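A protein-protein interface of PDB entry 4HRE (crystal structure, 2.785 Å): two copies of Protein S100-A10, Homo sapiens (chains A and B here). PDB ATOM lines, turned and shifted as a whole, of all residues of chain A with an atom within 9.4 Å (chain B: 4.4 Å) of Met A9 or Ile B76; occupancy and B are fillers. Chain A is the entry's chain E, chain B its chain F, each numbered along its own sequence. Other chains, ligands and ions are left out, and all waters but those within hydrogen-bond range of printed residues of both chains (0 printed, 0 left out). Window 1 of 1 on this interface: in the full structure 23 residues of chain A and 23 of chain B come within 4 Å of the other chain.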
ATOM      1  N   SER A   3       6.218 -25.908 -24.131  1.00  0.00           N
ATOM      2  CA  SER A   3       7.560 -25.869 -23.574  1.00  0.00           C
ATOM      3  C   SER A   3       7.463 -25.477 -22.106  1.00  0.00           C
ATOM      4  O   SER A   3       6.459 -24.900 -21.679  1.00  0.00           O
ATOM      5  CB  SER A   3       8.427 -24.868 -24.334  1.00  0.00           C
ATOM      6  OG  SER A   3       7.968 -23.541 -24.139  1.00  0.00           O
ATOM      7  N   GLN A   4       8.488 -25.815 -21.333  1.00  0.00           N
ATOM      8  CA  GLN A   4       8.502 -25.503 -19.907  1.00  0.00           C
ATOM      9  C   GLN A   4       8.292 -24.020 -19.642  1.00  0.00           C
ATOM     10  O   GLN A   4       7.479 -23.652 -18.794  1.00  0.00           O
ATOM     11  CB  GLN A   4       9.802 -25.967 -19.263  1.00  0.00           C
ATOM     12  CG  GLN A   4      10.872 -26.353 -20.254  1.00  0.00           C
ATOM     13  CD  GLN A   4      11.484 -27.687 -19.917  1.00  0.00           C
ATOM     14  OE1 GLN A   4      11.860 -28.455 -20.805  1.00  0.00           O
ATOM     15  NE2 GLN A   4      11.579 -27.979 -18.624  1.00  0.00           N
ATOM     16  N   MET A   5       9.020 -23.178 -20.376  1.00  0.00           N
ATOM     17  CA  MET A   5       8.922 -21.723 -20.240  1.00  0.00           C
ATOM     18  C   MET A   5       7.482 -21.238 -20.322  1.00  0.00           C
ATOM     19  O   MET A   5       7.096 -20.283 -19.648  1.00  0.00           O
ATOM     20  CB  MET A   5       9.754 -21.021 -21.317  1.00  0.00           C
ATOM     21  CG  MET A   5      11.236 -20.971 -21.028  1.00  0.00           C
ATOM     22  SD  MET A   5      11.611 -19.877 -19.649  1.00  0.00           S
ATOM     23  CE  MET A   5      11.015 -18.312 -20.277  1.00  0.00           C
ATOM     24  N   GLU A   6       6.692 -21.910 -21.155  1.00  0.00           N
ATOM     25  CA  GLU A   6       5.284 -21.583 -21.330  1.00  0.00           C
ATOM     26  C   GLU A   6       4.478 -21.755 -20.042  1.00  0.00           C
ATOM     27  O   GLU A   6       3.843 -20.810 -19.578  1.00  0.00           O
ATOM     28  CB  GLU A   6       4.682 -22.410 -22.472  1.00  0.00           C
ATOM     29  CG  GLU A   6       4.680 -21.707 -23.822  1.00  0.00           C
ATOM     30  CD  GLU A   6       4.719 -22.681 -24.982  1.00  0.00           C
ATOM     31  OE1 GLU A   6       5.297 -23.773 -24.813  1.00  0.00           O
ATOM     32  OE2 GLU A   6       4.180 -22.356 -26.061  1.00  0.00           O
ATOM     33  N   HIS A   7       4.502 -22.950 -19.460  1.00  0.00           N
ATOM     34  CA  HIS A   7       3.729 -23.191 -18.244  1.00  0.00           C
ATOM     35  C   HIS A   7       4.372 -22.534 -17.022  1.00  0.00           C
ATOM     36  O   HIS A   7       3.734 -22.389 -15.980  1.00  0.00           O
ATOM     37  CB  HIS A   7       3.511 -24.687 -17.999  1.00  0.00           C
ATOM     38  CG  HIS A   7       2.416 -24.982 -17.020  1.00  0.00           C
ATOM     39  ND1 HIS A   7       1.206 -24.325 -17.036  1.00  0.00           N
ATOM     40  CD2 HIS A   7       2.350 -25.867 -15.994  1.00  0.00           C
ATOM     41  CE1 HIS A   7       0.441 -24.786 -16.065  1.00  0.00           C
ATOM     42  NE2 HIS A   7       1.109 -25.723 -15.418  1.00  0.00           N
ATOM     43  N   ALA A   8       5.636 -22.141 -17.160  1.00  0.00           N
ATOM     44  CA  ALA A   8       6.332 -21.397 -16.113  1.00  0.00           C
ATOM     45  C   ALA A   8       5.819 -19.960 -16.075  1.00  0.00           C
ATOM     46  O   ALA A   8       5.496 -19.420 -15.005  1.00  0.00           O
ATOM     47  CB  ALA A   8       7.829 -21.412 -16.366  1.00  0.00           C
ATOM     48  N   MET A   9       5.743 -19.355 -17.259  1.00  0.00           N
ATOM     49  CA  MET A   9       5.131 -18.044 -17.441  1.00  0.00           C
ATOM     50  C   MET A   9       3.675 -18.077 -16.995  1.00  0.00           C
ATOM     51  O   MET A   9       3.190 -17.146 -16.351  1.00  0.00           O
ATOM     52  CB  MET A   9       5.191 -17.626 -18.911  1.00  0.00           C
ATOM     53  CG  MET A   9       6.545 -17.139 -19.386  1.00  0.00           C
ATOM     54  SD  MET A   9       6.439 -16.572 -21.091  1.00  0.00           S
ATOM     55  CE  MET A   9       4.953 -15.572 -21.017  1.00  0.00           C
ATOM     56  N   GLU A  10       2.989 -19.159 -17.350  1.00  0.00           N
ATOM     57  CA  GLU A  10       1.599 -19.373 -16.960  1.00  0.00           C
ATOM     58  C   GLU A  10       1.432 -19.455 -15.443  1.00  0.00           C
ATOM     59  O   GLU A  10       0.481 -18.903 -14.884  1.00  0.00           O
ATOM     60  CB  GLU A  10       1.055 -20.643 -17.624  1.00  0.00           C
ATOM     61  CG  GLU A  10      -0.013 -21.378 -16.820  1.00  0.00           C
ATOM     62  CD  GLU A  10      -1.392 -20.746 -16.926  1.00  0.00           C
ATOM     63  OE1 GLU A  10      -1.491 -19.579 -17.359  1.00  0.00           O
ATOM     64  OE2 GLU A  10      -2.383 -21.421 -16.577  1.00  0.00           O
ATOM     65  N   THR A  11       2.356 -20.144 -14.780  1.00  0.00           N
ATOM     66  CA  THR A  11       2.327 -20.241 -13.326  1.00  0.00           C
ATOM     67  C   THR A  11       2.540 -18.860 -12.724  1.00  0.00           C
ATOM     68  O   THR A  11       1.853 -18.474 -11.781  1.00  0.00           O
ATOM     69  CB  THR A  11       3.399 -21.203 -12.789  1.00  0.00           C
ATOM     70  OG1 THR A  11       3.399 -22.402 -13.571  1.00  0.00           O
ATOM     71  CG2 THR A  11       3.123 -21.544 -11.332  1.00  0.00           C
ATOM     72  N   MET A  12       3.490 -18.120 -13.290  1.00  0.00           N
ATOM     73  CA  MET A  12       3.712 -16.726 -12.920  1.00  0.00           C
ATOM     74  C   MET A  12       2.395 -15.946 -13.012  1.00  0.00           C
ATOM     75  O   MET A  12       2.071 -15.148 -12.131  1.00  0.00           O
ATOM     76  CB  MET A  12       4.775 -16.112 -13.839  1.00  0.00           C
ATOM     77  CG  MET A  12       5.601 -15.005 -13.216  1.00  0.00           C
ATOM     78  SD  MET A  12       7.244 -14.880 -13.966  1.00  0.00           S
ATOM     79  CE  MET A  12       7.781 -16.590 -13.894  1.00  0.00           C
ATOM     80  N   MET A  13       1.644 -16.192 -14.085  1.00  0.00           N
ATOM     81  CA  MET A  13       0.313 -15.610 -14.278  1.00  0.00           C
ATOM     82  C   MET A  13      -0.732 -15.965 -13.210  1.00  0.00           C
ATOM     83  O   MET A  13      -1.142 -15.099 -12.436  1.00  0.00           O
ATOM     84  CB  MET A  13      -0.224 -15.924 -15.681  1.00  0.00           C
ATOM     85  CG  MET A  13       0.212 -14.931 -16.750  1.00  0.00           C
ATOM     86  SD  MET A  13      -0.364 -15.394 -18.392  1.00  0.00           S
ATOM     87  CE  MET A  13      -2.043 -15.901 -18.037  1.00  0.00           C
ATOM     88  N   PHE A  14      -1.159 -17.227 -13.165  1.00  0.00           N
ATOM     89  CA  PHE A  14      -2.294 -17.601 -12.314  1.00  0.00           C
ATOM     90  C   PHE A  14      -1.972 -17.800 -10.828  1.00  0.00           C
ATOM     91  O   PHE A  14      -2.888 -17.893 -10.010  1.00  0.00           O
ATOM     92  CB  PHE A  14      -3.084 -18.797 -12.886  1.00  0.00           C
ATOM     93  CG  PHE A  14      -2.479 -20.148 -12.583  1.00  0.00           C
ATOM     94  CD1 PHE A  14      -2.780 -20.815 -11.401  1.00  0.00           C
ATOM     95  CD2 PHE A  14      -1.640 -20.766 -13.497  1.00  0.00           C
ATOM     96  CE1 PHE A  14      -2.232 -22.059 -11.123  1.00  0.00           C
ATOM     97  CE2 PHE A  14      -1.091 -22.014 -13.228  1.00  0.00           C
ATOM     98  CZ  PHE A  14      -1.388 -22.661 -12.039  1.00  0.00           C
ATOM     99  N   THR A  15      -0.693 -17.867 -10.468  1.00  0.00           N
ATOM    100  CA  THR A  15      -0.341 -17.912  -9.051  1.00  0.00           C
ATOM    101  C   THR A  15      -0.659 -16.554  -8.416  1.00  0.00           C
ATOM    102  O   THR A  15      -1.025 -16.475  -7.245  1.00  0.00           O
ATOM    103  CB  THR A  15       1.141 -18.321  -8.809  1.00  0.00           C
ATOM    104  OG1 THR A  15       1.267 -18.985  -7.545  1.00  0.00           O
ATOM    105  CG2 THR A  15       2.066 -17.115  -8.847  1.00  0.00           C
ATOM    106  N   PHE A  16      -0.545 -15.494  -9.211  1.00  0.00           N
ATOM    107  CA  PHE A  16      -0.908 -14.156  -8.769  1.00  0.00           C
ATOM    108  C   PHE A  16      -2.422 -14.061  -8.628  1.00  0.00           C
ATOM    109  O   PHE A  16      -2.935 -13.264  -7.842  1.00  0.00           O
ATOM    110  CB  PHE A  16      -0.398 -13.122  -9.776  1.00  0.00           C
ATOM    111  CG  PHE A  16      -0.928 -11.720  -9.555  1.00  0.00           C
ATOM    112  CD1 PHE A  16      -0.269 -10.842  -8.707  1.00  0.00           C
ATOM    113  CD2 PHE A  16      -2.073 -11.275 -10.217  1.00  0.00           C
ATOM    114  CE1 PHE A  16      -0.745  -9.550  -8.510  1.00  0.00           C
ATOM    115  CE2 PHE A  16      -2.555  -9.985 -10.027  1.00  0.00           C
ATOM    116  CZ  PHE A  16      -1.890  -9.122  -9.171  1.00  0.00           C
ATOM    117  N   HIS A  17      -3.131 -14.888  -9.391  1.00  0.00           N
ATOM    118  CA  HIS A  17      -4.588 -14.815  -9.465  1.00  0.00           C
ATOM    119  C   HIS A  17      -5.322 -15.500  -8.320  1.00  0.00           C
ATOM    120  O   HIS A  17      -6.514 -15.271  -8.124  1.00  0.00           O
ATOM    121  CB  HIS A  17      -5.091 -15.351 -10.805  1.00  0.00           C
ATOM    122  CG  HIS A  17      -5.229 -14.302 -11.856  1.00  0.00           C
ATOM    123  ND1 HIS A  17      -4.143 -13.685 -12.445  1.00  0.00           N
ATOM    124  CD2 HIS A  17      -6.329 -13.743 -12.422  1.00  0.00           C
ATOM    125  CE1 HIS A  17      -4.571 -12.801 -13.327  1.00  0.00           C
ATOM    126  NE2 HIS A  17      -5.884 -12.816 -13.334  1.00  0.00           N
ATOM    127  N   PHE A  69      -0.447  -6.852 -11.282  1.00  0.00           N
ATOM    128  CA  PHE A  69       0.399  -7.952 -11.721  1.00  0.00           C
ATOM    129  C   PHE A  69       1.772  -7.415 -12.103  1.00  0.00           C
ATOM    130  O   PHE A  69       2.782  -8.095 -11.927  1.00  0.00           O
ATOM    131  CB  PHE A  69      -0.237  -8.686 -12.900  1.00  0.00           C
ATOM    132  CG  PHE A  69       0.440  -9.988 -13.246  1.00  0.00           C
ATOM    133  CD1 PHE A  69       1.516 -10.023 -14.123  1.00  0.00           C
ATOM    134  CD2 PHE A  69      -0.008 -11.176 -12.703  1.00  0.00           C
ATOM    135  CE1 PHE A  69       2.130 -11.223 -14.441  1.00  0.00           C
ATOM    136  CE2 PHE A  69       0.597 -12.375 -13.016  1.00  0.00           C
ATOM    137  CZ  PHE A  69       1.669 -12.401 -13.884  1.00  0.00           C
ATOM    138  N   PHE A  72       3.788  -7.160  -8.680  1.00  0.00           N
ATOM    139  CA  PHE A  72       4.150  -8.496  -8.234  1.00  0.00           C
ATOM    140  C   PHE A  72       5.285  -9.034  -9.110  1.00  0.00           C
ATOM    141  O   PHE A  72       6.256  -9.643  -8.632  1.00  0.00           O
ATOM    142  CB  PHE A  72       2.909  -9.387  -8.298  1.00  0.00           C
ATOM    143  CG  PHE A  72       3.191 -10.815  -8.653  1.00  0.00           C
ATOM    144  CD1 PHE A  72       3.611 -11.711  -7.687  1.00  0.00           C
ATOM    145  CD2 PHE A  72       3.005 -11.269  -9.950  1.00  0.00           C
ATOM    146  CE1 PHE A  72       3.864 -13.036  -8.008  1.00  0.00           C
ATOM    147  CE2 PHE A  72       3.255 -12.594 -10.280  1.00  0.00           C
ATOM    148  CZ  PHE A  72       3.680 -13.480  -9.305  1.00  0.00           C
ATOM    149  N   PHE A  73       5.167  -8.764 -10.402  1.00  0.00           N
ATOM    150  CA  PHE A  73       6.188  -9.164 -11.349  1.00  0.00           C
ATOM    151  C   PHE A  73       7.472  -8.391 -11.110  1.00  0.00           C
ATOM    152  O   PHE A  73       8.549  -8.869 -11.438  1.00  0.00           O
ATOM    153  CB  PHE A  73       5.709  -8.937 -12.774  1.00  0.00           C
ATOM    154  CG  PHE A  73       6.263  -9.917 -13.758  1.00  0.00           C
ATOM    155  CD1 PHE A  73       7.568  -9.805 -14.221  1.00  0.00           C
ATOM    156  CD2 PHE A  73       5.477 -10.958 -14.226  1.00  0.00           C
ATOM    157  CE1 PHE A  73       8.076 -10.717 -15.145  1.00  0.00           C
ATOM    158  CE2 PHE A  73       5.972 -11.871 -15.148  1.00  0.00           C
ATOM    159  CZ  PHE A  73       7.274 -11.753 -15.609  1.00  0.00           C
ATOM    160  N   ILE A  76       9.148 -10.378  -8.569  1.00  0.00           N
ATOM    161  CA  ILE A  76       9.852 -11.451  -9.258  1.00  0.00           C
ATOM    162  C   ILE A  76      11.117 -10.954  -9.946  1.00  0.00           C
ATOM    163  O   ILE A  76      12.102 -11.670 -10.035  1.00  0.00           O
ATOM    164  CB  ILE A  76       8.968 -12.151 -10.296  1.00  0.00           C
ATOM    165  CG1 ILE A  76       7.563 -12.358  -9.733  1.00  0.00           C
ATOM    166  CG2 ILE A  76       9.599 -13.480 -10.720  1.00  0.00           C
ATOM    167  CD1 ILE A  76       6.861 -13.535 -10.326  1.00  0.00           C
ATOM    168  N   PHE B  39       8.523 -20.964 -27.920  1.00  0.00           N
ATOM    169  CA  PHE B  39       7.196 -20.683 -28.467  1.00  0.00           C
ATOM    170  C   PHE B  39       7.157 -20.861 -29.980  1.00  0.00           C
ATOM    171  O   PHE B  39       7.109 -19.870 -30.716  1.00  0.00           O
ATOM    172  CB  PHE B  39       6.743 -19.259 -28.130  1.00  0.00           C
ATOM    173  CG  PHE B  39       7.478 -18.640 -26.978  1.00  0.00           C
ATOM    174  CD1 PHE B  39       7.068 -18.866 -25.673  1.00  0.00           C
ATOM    175  CD2 PHE B  39       8.571 -17.818 -27.201  1.00  0.00           C
ATOM    176  CE1 PHE B  39       7.740 -18.291 -24.607  1.00  0.00           C
ATOM    177  CE2 PHE B  39       9.250 -17.236 -26.141  1.00  0.00           C
ATOM    178  CZ  PHE B  39       8.834 -17.474 -24.841  1.00  0.00           C
ATOM    179  N   PHE B  72      16.585  -9.989 -20.850  1.00  0.00           N
ATOM    180  CA  PHE B  72      15.841 -11.209 -21.173  1.00  0.00           C
ATOM    181  C   PHE B  72      14.563 -11.310 -20.337  1.00  0.00           C
ATOM    182  O   PHE B  72      13.501 -11.707 -20.824  1.00  0.00           O
ATOM    183  CB  PHE B  72      16.746 -12.434 -20.973  1.00  0.00           C
ATOM    184  CG  PHE B  72      16.004 -13.714 -20.693  1.00  0.00           C
ATOM    185  CD1 PHE B  72      15.429 -14.444 -21.726  1.00  0.00           C
ATOM    186  CD2 PHE B  72      15.911 -14.203 -19.394  1.00  0.00           C
ATOM    187  CE1 PHE B  72      14.752 -15.631 -21.469  1.00  0.00           C
ATOM    188  CE2 PHE B  72      15.237 -15.388 -19.127  1.00  0.00           C
ATOM    189  CZ  PHE B  72      14.655 -16.106 -20.172  1.00  0.00           C
ATOM    190  N   PHE B  73      14.683 -10.934 -19.071  1.00  0.00           N
ATOM    191  CA  PHE B  73      13.552 -10.874 -18.167  1.00  0.00           C
ATOM    192  C   PHE B  73      12.647  -9.735 -18.617  1.00  0.00           C
ATOM    193  O   PHE B  73      11.423  -9.843 -18.567  1.00  0.00           O
ATOM    194  CB  PHE B  73      14.061 -10.621 -16.744  1.00  0.00           C
ATOM    195  CG  PHE B  73      13.106 -11.040 -15.664  1.00  0.00           C
ATOM    196  CD1 PHE B  73      12.158 -10.152 -15.171  1.00  0.00           C
ATOM    197  CD2 PHE B  73      13.166 -12.320 -15.128  1.00  0.00           C
ATOM    198  CE1 PHE B  73      11.278 -10.538 -14.168  1.00  0.00           C
ATOM    199  CE2 PHE B  73      12.290 -12.717 -14.126  1.00  0.00           C
ATOM    200  CZ  PHE B  73      11.344 -11.827 -13.644  1.00  0.00           C
ATOM    201  N   SER B  74      13.269  -8.643 -19.052  1.00  0.00           N
ATOM    202  CA  SER B  74      12.555  -7.479 -19.561  1.00  0.00           C
ATOM    203  C   SER B  74      11.640  -7.869 -20.722  1.00  0.00           C
ATOM    204  O   SER B  74      10.511  -7.385 -20.821  1.00  0.00           O
ATOM    205  CB  SER B  74      13.554  -6.400 -19.989  1.00  0.00           C
ATOM    206  OG  SER B  74      12.940  -5.396 -20.773  1.00  0.00           O
ATOM    207  N   LEU B  75      12.134  -8.744 -21.594  1.00  0.00           N
ATOM    208  CA  LEU B  75      11.319  -9.327 -22.661  1.00  0.00           C
ATOM    209  C   LEU B  75      10.100 -10.087 -22.130  1.00  0.00           C
ATOM    210  O   LEU B  75       8.959  -9.668 -22.333  1.00  0.00           O
ATOM    211  CB  LEU B  75      12.160 -10.260 -23.538  1.00  0.00           C
ATOM    212  CG  LEU B  75      11.364 -11.005 -24.611  1.00  0.00           C
ATOM    213  CD1 LEU B  75      11.435 -10.259 -25.934  1.00  0.00           C
ATOM    214  CD2 LEU B  75      11.841 -12.450 -24.742  1.00  0.00           C
ATOM    215  N   ILE B  76      10.353 -11.201 -21.450  1.00  0.00           N
ATOM    216  CA  ILE B  76       9.286 -12.031 -20.904  1.00  0.00           C
ATOM    217  C   ILE B  76       8.231 -11.198 -20.181  1.00  0.00           C
ATOM    218  O   ILE B  76       7.036 -11.479 -20.276  1.00  0.00           O
ATOM    219  CB  ILE B  76       9.838 -13.093 -19.934  1.00  0.00           C
ATOM    220  CG1 ILE B  76      10.809 -14.026 -20.661  1.00  0.00           C
ATOM    221  CG2 ILE B  76       8.701 -13.884 -19.305  1.00  0.00           C
ATOM    222  CD1 ILE B  76      10.293 -14.526 -21.992  1.00  0.00           C
ATOM    223  N   ALA B  77       8.681 -10.176 -19.459  1.00  0.00           N
ATOM    224  CA  ALA B  77       7.775  -9.306 -18.717  1.00  0.00           C
ATOM    225  C   ALA B  77       6.569  -8.912 -19.562  1.00  0.00           C
ATOM    226  O   ALA B  77       5.424  -9.118 -19.161  1.00  0.00           O
ATOM    227  CB  ALA B  77       8.513  -8.066 -18.231  1.00  0.00           C
ATOM    228  N   GLY B  78       6.836  -8.346 -20.734  1.00  0.00           N
ATOM    229  CA  GLY B  78       5.782  -7.939 -21.647  1.00  0.00           C
ATOM    230  C   GLY B  78       4.835  -9.055 -22.050  1.00  0.00           C
ATOM    231  O   GLY B  78       3.611  -8.873 -22.013  1.00  0.00           O
ATOM    232  N   LEU B  79       5.389 -10.209 -22.427  1.00  0.00           N
ATOM    233  CA  LEU B  79       4.566 -11.357 -22.807  1.00  0.00           C
ATOM    234  C   LEU B  79       3.678 -11.792 -21.638  1.00  0.00           C
ATOM    235  O   LEU B  79       2.454 -11.860 -21.769  1.00  0.00           O
ATOM    236  CB  LEU B  79       5.418 -12.538 -23.317  1.00  0.00           C
ATOM    237  CG  LEU B  79       6.017 -12.537 -24.738  1.00  0.00           C
ATOM    238  CD1 LEU B  79       7.407 -11.911 -24.786  1.00  0.00           C
ATOM    239  CD2 LEU B  79       6.066 -13.952 -25.292  1.00  0.00           C
ATOM    240  N   THR B  80       4.302 -12.051 -20.490  1.00  0.00           N
ATOM    241  CA  THR B  80       3.604 -12.583 -19.320  1.00  0.00           C
ATOM    242  C   THR B  80       2.514 -11.643 -18.802  1.00  0.00           C
ATOM    243  O   THR B  80       1.468 -12.100 -18.340  1.00  0.00           O
ATOM    244  CB  THR B  80       4.587 -12.922 -18.168  1.00  0.00           C
ATOM    245  OG1 THR B  80       5.919 -13.047 -18.681  1.00  0.00           O
ATOM    246  CG2 THR B  80       4.194 -14.224 -17.486  1.00  0.00           C
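Of chain B, only Ile B76, Leu B79 and Thr B80 come within 4 Å of Met A9.
Of chain A, only Met A9 comes within 4 Å of Ile B76.
No residue of chain A comes within 4 Å of Leu B75.
No residue of chain A comes within 4 Å of Gly B78.
Leu B79 touches one residue of chain A.
Of the printed residues of chain B, Met A13 touches Thr B80.
Printed residues of chain B within 4 Å of Phe A73: Phe B73, Ala B77 and Thr B80.
Of the printed residues of chain B, Ile A76 touches Phe B73.
Printed residues of chain A within 4 Å of Phe B73: Phe A73 (3.4 Å) and Ile A76 (3.7 Å).
Thr A11 touches none of the printed residues of chain B.
His A17 touches none of the printed residues of chain B.
The nearest residue of chain A that does not touch Ile B76 is Met A5 (4.2 Å).
The nearest printed residue of chain B that does not touch Phe A73 is Ile B76 (4.5 Å).
OG1 of Thr B80 is in hydrogen-bond range of O of Ile B76.
The backbone carbonyl oxygen (O) of Met A13 sits at hydrogen-bond distance from a ring nitrogen (ND1) of His A17 (3.3 Å).
Of the 10 printed residues of chain B, 5 touch a printed residue of chain A.
Printed residues of chain B that touch a printed residue of chain A: Phe B73, Ile B76, Ala B77, Leu B79 and Thr B80.
Hydrophobic or aromatic side chains of chain B within 4 Å of the printed part of chain A: Phe B73, Ile B76 and Leu B79.
Along chain B the printed residues that touch a printed residue of chain A span positions 73 to 80.
Of the 19 printed residues of chain A, 4 touch a printed residue of chain B.
Hydrophobic or aromatic side chains of chain A within 4 Å of the printed part of chain B: Met A9, Met A13, Phe A73 and Ile A76.
Among the printed residues, 8 pairs touch across the chains.
The backbone carbonyl oxygen (O) of Thr B80 lies close to the side-chain sulfur (SD) of Met A13 (3.8 Å).
Met A9 touches Ile B76.
Met A9 touches Leu B79 (CE to CB, 3.8 Å).
Met A9 touches Thr B80.
CE1 of Phe A73 touches CE1 of Phe B73 (3.4 Å).
Phe A73 touches Ala B77 (CE1 to CA, 3.9 Å).
Thr B80 touches Phe A73 (CB to CE2, 3.5 Å).
Ile A76 touches Phe B73.
Phe B73 touches its own counterpart, Phe A73.
Ile A76 touches Phe B73, but with the chains exchanged Phe A73 does not touch Ile B76 (4.5 Å).
3 positions are printed for both chains.
Of the 8 pairs that touch across the chains among the printed residues, 1 has its exchanged pair printed and touching as well.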
